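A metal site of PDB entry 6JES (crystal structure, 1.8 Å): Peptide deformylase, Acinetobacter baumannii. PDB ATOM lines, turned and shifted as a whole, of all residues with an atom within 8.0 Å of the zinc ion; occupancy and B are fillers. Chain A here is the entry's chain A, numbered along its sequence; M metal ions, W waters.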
ATOM      1  N   VAL A   6     -10.769  11.710   4.230  1.00  0.00           N
ATOM      2  CA  VAL A   6      -9.349  11.802   3.906  1.00  0.00           C
ATOM      3  C   VAL A   6      -9.029  10.689   2.954  1.00  0.00           C
ATOM      4  O   VAL A   6      -9.369   9.525   3.172  1.00  0.00           O
ATOM      5  CB  VAL A   6      -8.490  11.726   5.194  1.00  0.00           C
ATOM      6  CG1 VAL A   6      -7.002  11.499   4.873  1.00  0.00           C
ATOM      7  CG2 VAL A   6      -8.723  12.937   6.075  1.00  0.00           C
ATOM      8  N   LEU A  14      -4.274  11.794  -4.806  1.00  0.00           N
ATOM      9  CA  LEU A  14      -3.020  12.048  -4.082  1.00  0.00           C
ATOM     10  C   LEU A  14      -1.798  12.085  -4.973  1.00  0.00           C
ATOM     11  O   LEU A  14      -0.731  12.437  -4.535  1.00  0.00           O
ATOM     12  CB  LEU A  14      -2.825  10.999  -3.026  1.00  0.00           C
ATOM     13  CG  LEU A  14      -3.289  11.090  -1.587  1.00  0.00           C
ATOM     14  CD1 LEU A  14      -3.984  12.342  -1.073  1.00  0.00           C
ATOM     15  CD2 LEU A  14      -3.811   9.788  -1.059  1.00  0.00           C
ATOM     16  N   GLY A  49       0.134  18.337  10.364  1.00  0.00           N
ATOM     17  CA  GLY A  49      -0.014  19.141   9.193  1.00  0.00           C
ATOM     18  C   GLY A  49      -1.060  18.488   8.318  1.00  0.00           C
ATOM     19  O   GLY A  49      -1.501  17.311   8.571  1.00  0.00           O
ATOM     20  N   ILE A  50      -1.480  19.173   7.272  1.00  0.00           N
ATOM     21  CA  ILE A  50      -2.469  18.620   6.319  1.00  0.00           C
ATOM     22  C   ILE A  50      -2.353  19.399   5.041  1.00  0.00           C
ATOM     23  O   ILE A  50      -1.931  20.545   5.054  1.00  0.00           O
ATOM     24  CB  ILE A  50      -3.909  18.605   6.856  1.00  0.00           C
ATOM     25  CG1 ILE A  50      -4.840  17.661   6.016  1.00  0.00           C
ATOM     26  CG2 ILE A  50      -4.479  19.990   7.065  1.00  0.00           C
ATOM     27  CD1 ILE A  50      -6.169  17.405   6.702  1.00  0.00           C
ATOM     28  N   ALA A  51      -2.697  18.750   3.926  1.00  0.00           N
ATOM     29  CA  ALA A  51      -2.670  19.341   2.589  1.00  0.00           C
ATOM     30  C   ALA A  51      -4.026  19.133   1.949  1.00  0.00           C
ATOM     31  O   ALA A  51      -4.684  18.077   2.153  1.00  0.00           O
ATOM     32  CB  ALA A  51      -1.552  18.686   1.771  1.00  0.00           C
ATOM     33  N   GLN A  54      -5.447  15.845   0.340  1.00  0.00           N
ATOM     34  CA  GLN A  54      -5.800  14.813   1.268  1.00  0.00           C
ATOM     35  C   GLN A  54      -7.264  14.807   1.573  1.00  0.00           C
ATOM     36  O   GLN A  54      -7.767  13.766   2.002  1.00  0.00           O
ATOM     37  CB  GLN A  54      -4.995  14.862   2.594  1.00  0.00           C
ATOM     38  CG  GLN A  54      -3.544  14.636   2.409  1.00  0.00           C
ATOM     39  CD  GLN A  54      -2.831  14.692   3.713  1.00  0.00           C
ATOM     40  OE1 GLN A  54      -2.438  15.794   4.151  1.00  0.00           O
ATOM     41  NE2 GLN A  54      -2.666  13.504   4.393  1.00  0.00           N
ATOM     42  N   ARG A  71       0.236  10.587  18.282  1.00  0.00           N
ATOM     43  CA  ARG A  71       0.992  10.234  17.071  1.00  0.00           C
ATOM     44  C   ARG A  71       2.422  10.772  17.064  1.00  0.00           C
ATOM     45  O   ARG A  71       3.343  10.092  16.535  1.00  0.00           O
ATOM     46  CB  ARG A  71       0.222  10.673  15.828  1.00  0.00           C
ATOM     47  CG  ARG A  71      -1.207  10.140  15.778  1.00  0.00           C
ATOM     48  CD  ARG A  71      -1.903  10.307  14.425  1.00  0.00           C
ATOM     49  NE  ARG A  71      -1.098   9.924  13.245  1.00  0.00           N
ATOM     50  CZ  ARG A  71      -0.486  10.774  12.401  1.00  0.00           C
ATOM     51  NH1 ARG A  71      -0.531  12.087  12.563  1.00  0.00           N
ATOM     52  NH2 ARG A  71       0.197  10.299  11.395  1.00  0.00           N
ATOM     53  N   TYR A  72       2.629  11.988  17.616  1.00  0.00           N
ATOM     54  CA  TYR A  72       3.998  12.572  17.753  1.00  0.00           C
ATOM     55  C   TYR A  72       4.186  13.122  19.174  1.00  0.00           C
ATOM     56  O   TYR A  72       3.913  14.325  19.430  1.00  0.00           O
ATOM     57  CB  TYR A  72       4.250  13.660  16.697  1.00  0.00           C
ATOM     58  CG  TYR A  72       4.145  13.165  15.262  1.00  0.00           C
ATOM     59  CD1 TYR A  72       5.223  12.578  14.657  1.00  0.00           C
ATOM     60  CD2 TYR A  72       2.963  13.288  14.540  1.00  0.00           C
ATOM     61  CE1 TYR A  72       5.153  12.118  13.352  1.00  0.00           C
ATOM     62  CE2 TYR A  72       2.893  12.873  13.215  1.00  0.00           C
ATOM     63  CZ  TYR A  72       3.978  12.283  12.622  1.00  0.00           C
ATOM     64  OH  TYR A  72       3.924  11.808  11.288  1.00  0.00           O
ATOM     65  N   GLU A 100       8.359   9.611  10.027  1.00  0.00           N
ATOM     66  CA  GLU A 100       7.101  10.243   9.611  1.00  0.00           C
ATOM     67  C   GLU A 100       5.996   9.195   9.457  1.00  0.00           C
ATOM     68  O   GLU A 100       6.239   8.096   9.013  1.00  0.00           O
ATOM     69  CB  GLU A 100       7.271  10.961   8.263  1.00  0.00           C
ATOM     70  CG  GLU A 100       8.378  11.987   8.294  1.00  0.00           C
ATOM     71  CD  GLU A 100       8.480  12.818   7.021  1.00  0.00           C
ATOM     72  OE1 GLU A 100       7.542  12.817   6.158  1.00  0.00           O
ATOM     73  OE2 GLU A 100       9.500  13.523   6.875  1.00  0.00           O
ATOM     74  N   GLY A 101       4.787   9.611   9.809  1.00  0.00           N
ATOM     75  CA  GLY A 101       3.528   8.975   9.391  1.00  0.00           C
ATOM     76  C   GLY A 101       2.798   9.935   8.437  1.00  0.00           C
ATOM     77  O   GLY A 101       3.363  10.943   7.958  1.00  0.00           O
ATOM     78  N   CYS A 102       1.554   9.603   8.142  1.00  0.00           N
ATOM     79  CA  CYS A 102       0.744  10.481   7.259  1.00  0.00           C
ATOM     80  C   CYS A 102      -0.721  10.118   7.413  1.00  0.00           C
ATOM     81  O   CYS A 102      -1.055   8.936   7.549  1.00  0.00           O
ATOM     82  CB  CYS A 102       1.249  10.362   5.815  1.00  0.00           C
ATOM     83  SG  CYS A 102       0.130  11.081   4.596  1.00  0.00           S
ATOM     84  N   LEU A 103      -1.618  11.103   7.373  1.00  0.00           N
ATOM     85  CA  LEU A 103      -3.049  10.807   7.567  1.00  0.00           C
ATOM     86  C   LEU A 103      -3.615   9.921   6.446  1.00  0.00           C
ATOM     87  O   LEU A 103      -4.630   9.304   6.636  1.00  0.00           O
ATOM     88  CB  LEU A 103      -3.869  12.078   7.693  1.00  0.00           C
ATOM     89  CG  LEU A 103      -3.356  13.145   8.692  1.00  0.00           C
ATOM     90  CD1 LEU A 103      -4.346  14.282   8.817  1.00  0.00           C
ATOM     91  CD2 LEU A 103      -3.107  12.532  10.072  1.00  0.00           C
ATOM     92  N   SER A 104      -2.926   9.888   5.329  1.00  0.00           N
ATOM     93  CA  SER A 104      -3.302   9.176   4.142  1.00  0.00           C
ATOM     94  C   SER A 104      -2.606   7.800   4.024  1.00  0.00           C
ATOM     95  O   SER A 104      -2.831   7.067   3.062  1.00  0.00           O
ATOM     96  CB  SER A 104      -2.973  10.062   2.908  1.00  0.00           C
ATOM     97  OG  SER A 104      -3.862  11.204   2.872  1.00  0.00           O
ATOM     98  N   VAL A 105      -1.781   7.466   5.007  1.00  0.00           N
ATOM     99  CA  VAL A 105      -1.091   6.165   5.020  1.00  0.00           C
ATOM    100  C   VAL A 105      -1.379   5.481   6.391  1.00  0.00           C
ATOM    101  O   VAL A 105      -0.552   5.495   7.349  1.00  0.00           O
ATOM    102  CB  VAL A 105       0.414   6.331   4.718  1.00  0.00           C
ATOM    103  CG1 VAL A 105       1.068   4.950   4.621  1.00  0.00           C
ATOM    104  CG2 VAL A 105       0.616   7.080   3.410  1.00  0.00           C
ATOM    105  N   ARG A 114      15.171  14.611   5.209  1.00  0.00           N
ATOM    106  CA  ARG A 114      14.599  15.892   4.806  1.00  0.00           C
ATOM    107  C   ARG A 114      15.690  16.895   5.014  1.00  0.00           C
ATOM    108  O   ARG A 114      16.622  16.653   5.782  1.00  0.00           O
ATOM    109  CB  ARG A 114      13.449  16.246   5.720  1.00  0.00           C
ATOM    110  CG  ARG A 114      12.257  15.289   5.621  1.00  0.00           C
ATOM    111  CD  ARG A 114      11.542  15.420   4.227  1.00  0.00           C
ATOM    112  NE  ARG A 114      10.272  14.757   4.337  1.00  0.00           N
ATOM    113  CZ  ARG A 114       9.370  14.626   3.405  1.00  0.00           C
ATOM    114  NH1 ARG A 114       9.575  15.122   2.244  1.00  0.00           N
ATOM    115  NH2 ARG A 114       8.242  13.938   3.663  1.00  0.00           N
ATOM    116  N   ILE A 141       7.682  18.954   8.267  1.00  0.00           N
ATOM    117  CA  ILE A 141       6.234  19.003   7.967  1.00  0.00           C
ATOM    118  C   ILE A 141       6.012  19.837   6.696  1.00  0.00           C
ATOM    119  O   ILE A 141       5.260  19.404   5.802  1.00  0.00           O
ATOM    120  CB  ILE A 141       5.409  19.598   9.138  1.00  0.00           C
ATOM    121  CG1 ILE A 141       5.515  18.693  10.379  1.00  0.00           C
ATOM    122  CG2 ILE A 141       3.953  19.774   8.769  1.00  0.00           C
ATOM    123  CD1 ILE A 141       5.099  19.354  11.677  1.00  0.00           C
ATOM    124  N   HIS A 144       6.900  17.622   3.753  1.00  0.00           N
ATOM    125  CA  HIS A 144       5.874  16.587   3.642  1.00  0.00           C
ATOM    126  C   HIS A 144       4.607  17.136   2.954  1.00  0.00           C
ATOM    127  O   HIS A 144       4.087  16.552   2.010  1.00  0.00           O
ATOM    128  CB  HIS A 144       5.605  16.003   5.021  1.00  0.00           C
ATOM    129  CG  HIS A 144       4.590  14.906   5.045  1.00  0.00           C
ATOM    130  ND1 HIS A 144       4.897  13.617   5.474  1.00  0.00           N
ATOM    131  CD2 HIS A 144       3.244  14.918   4.812  1.00  0.00           C
ATOM    132  CE1 HIS A 144       3.809  12.879   5.433  1.00  0.00           C
ATOM    133  NE2 HIS A 144       2.792  13.642   5.037  1.00  0.00           N
ATOM    134  N   GLU A 145       4.133  18.294   3.415  1.00  0.00           N
ATOM    135  CA  GLU A 145       2.937  18.834   2.851  1.00  0.00           C
ATOM    136  C   GLU A 145       3.121  19.377   1.458  1.00  0.00           C
ATOM    137  O   GLU A 145       2.220  19.214   0.615  1.00  0.00           O
ATOM    138  CB  GLU A 145       2.377  19.945   3.767  1.00  0.00           C
ATOM    139  CG  GLU A 145       2.099  19.496   5.203  1.00  0.00           C
ATOM    140  CD  GLU A 145       1.184  18.311   5.323  1.00  0.00           C
ATOM    141  OE1 GLU A 145       0.358  18.077   4.471  1.00  0.00           O
ATOM    142  OE2 GLU A 145       1.307  17.575   6.310  1.00  0.00           O
ATOM    143  N   ASP A 147       5.173  18.143  -0.613  1.00  0.00           N
ATOM    144  CA  ASP A 147       5.156  16.874  -1.398  1.00  0.00           C
ATOM    145  C   ASP A 147       3.731  16.452  -1.718  1.00  0.00           C
ATOM    146  O   ASP A 147       3.405  16.137  -2.862  1.00  0.00           O
ATOM    147  CB  ASP A 147       5.894  15.720  -0.648  1.00  0.00           C
ATOM    148  CG  ASP A 147       7.356  15.702  -0.834  1.00  0.00           C
ATOM    149  OD1 ASP A 147       7.930  16.489  -1.583  1.00  0.00           O
ATOM    150  OD2 ASP A 147       7.996  14.856  -0.140  1.00  0.00           O
ATOM    151  N   HIS A 148       2.798  16.561  -0.796  1.00  0.00           N
ATOM    152  CA  HIS A 148       1.424  16.178  -1.101  1.00  0.00           C
ATOM    153  C   HIS A 148       0.842  17.015  -2.258  1.00  0.00           C
ATOM    154  O   HIS A 148       0.071  16.528  -3.058  1.00  0.00           O
ATOM    155  CB  HIS A 148       0.461  16.358   0.087  1.00  0.00           C
ATOM    156  CG  HIS A 148       0.413  15.223   1.078  1.00  0.00           C
ATOM    157  ND1 HIS A 148       0.067  13.944   0.725  1.00  0.00           N
ATOM    158  CD2 HIS A 148       0.590  15.222   2.418  1.00  0.00           C
ATOM    159  CE1 HIS A 148       0.113  13.177   1.803  1.00  0.00           C
ATOM    160  NE2 HIS A 148       0.352  13.937   2.846  1.00  0.00           N
ATOM    161  N   ILE A 152       3.186  13.455  -4.139  1.00  0.00           N
ATOM    162  CA  ILE A 152       4.283  12.622  -3.531  1.00  0.00           C
ATOM    163  C   ILE A 152       3.916  12.250  -2.110  1.00  0.00           C
ATOM    164  O   ILE A 152       3.547  13.101  -1.299  1.00  0.00           O
ATOM    165  CB  ILE A 152       5.625  13.347  -3.533  1.00  0.00           C
ATOM    166  CG1 ILE A 152       6.132  13.544  -4.961  1.00  0.00           C
ATOM    167  CG2 ILE A 152       6.656  12.596  -2.736  1.00  0.00           C
ATOM    168  CD1 ILE A 152       7.125  14.664  -5.074  1.00  0.00           C
ATOM    169  N   LEU A 153       4.007  10.946  -1.791  1.00  0.00           N
ATOM    170  CA  LEU A 153       3.727  10.464  -0.461  1.00  0.00           C
ATOM    171  C   LEU A 153       5.078  10.040   0.148  1.00  0.00           C
ATOM    172  O   LEU A 153       6.026   9.719  -0.598  1.00  0.00           O
ATOM    173  CB  LEU A 153       2.798   9.226  -0.488  1.00  0.00           C
ATOM    174  CG  LEU A 153       1.400   9.434  -1.112  1.00  0.00           C
ATOM    175  CD1 LEU A 153       0.601   8.155  -1.113  1.00  0.00           C
ATOM    176  CD2 LEU A 153       0.661  10.478  -0.290  1.00  0.00           C
ATOM    177  N   PHE A 154       5.164  10.078   1.474  1.00  0.00           N
ATOM    178  CA  PHE A 154       6.467   9.977   2.185  1.00  0.00           C
ATOM    179  C   PHE A 154       7.088   8.631   1.942  1.00  0.00           C
ATOM    180  O   PHE A 154       8.323   8.517   1.944  1.00  0.00           O
ATOM    181  CB  PHE A 154       6.329  10.254   3.702  1.00  0.00           C
ATOM    182  CG  PHE A 154       5.821   9.046   4.512  1.00  0.00           C
ATOM    183  CD1 PHE A 154       6.723   8.130   5.046  1.00  0.00           C
ATOM    184  CD2 PHE A 154       4.446   8.845   4.709  1.00  0.00           C
ATOM    185  CE1 PHE A 154       6.252   7.032   5.764  1.00  0.00           C
ATOM    186  CE2 PHE A 154       3.978   7.752   5.419  1.00  0.00           C
ATOM    187  CZ  PHE A 154       4.889   6.838   5.957  1.00  0.00           C
HETATM  188 ZN    ZN M   1       0.786  13.211   4.807  1.00  0.00          ZN
HETATM  189  O   HOH W   1       0.200  15.181   6.069  1.00  0.00           O
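ND1 of His 144 sits at hydrogen-bond distance from OE1 of Glu 100.
NE2 of His 148 lies close to NE2 of Gln 54.
SG of Cys 102 sits close to NE2 of Gln 54 (3.7 Å).
N of Ser 104 lies close to SG of Cys 102 (3.4 Å).
The side-chain hydroxyl (OG) of Ser 104 sits at hydrogen-bond distance from the side-chain amide nitrogen (NE2) of Gln 54, 3.0 Å away.
The backbone NH (N) of Ala 51 sits at hydrogen-bond distance from the side-chain amide oxygen (OE1) of Gln 54, 3.0 Å away.
NE2 of Gln 54 touches the zinc ion, 3.5 Å away.
The nearest printed residue that does not touch the zinc ion is Leu 103 (4.1 Å).
The zinc ion is bound by NE2 of His 144 (2.1 Å), NE2 of His 148 (2.1 Å), SG of Cys 102 (2.2 Å) and water W1 (2.4 Å).
The zinc ion has four donor atoms within binding distance.
Water W1 bridges OE2 of Glu 145 (2.6 Å) and OE1 of Gln 54 (3.3 Å).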
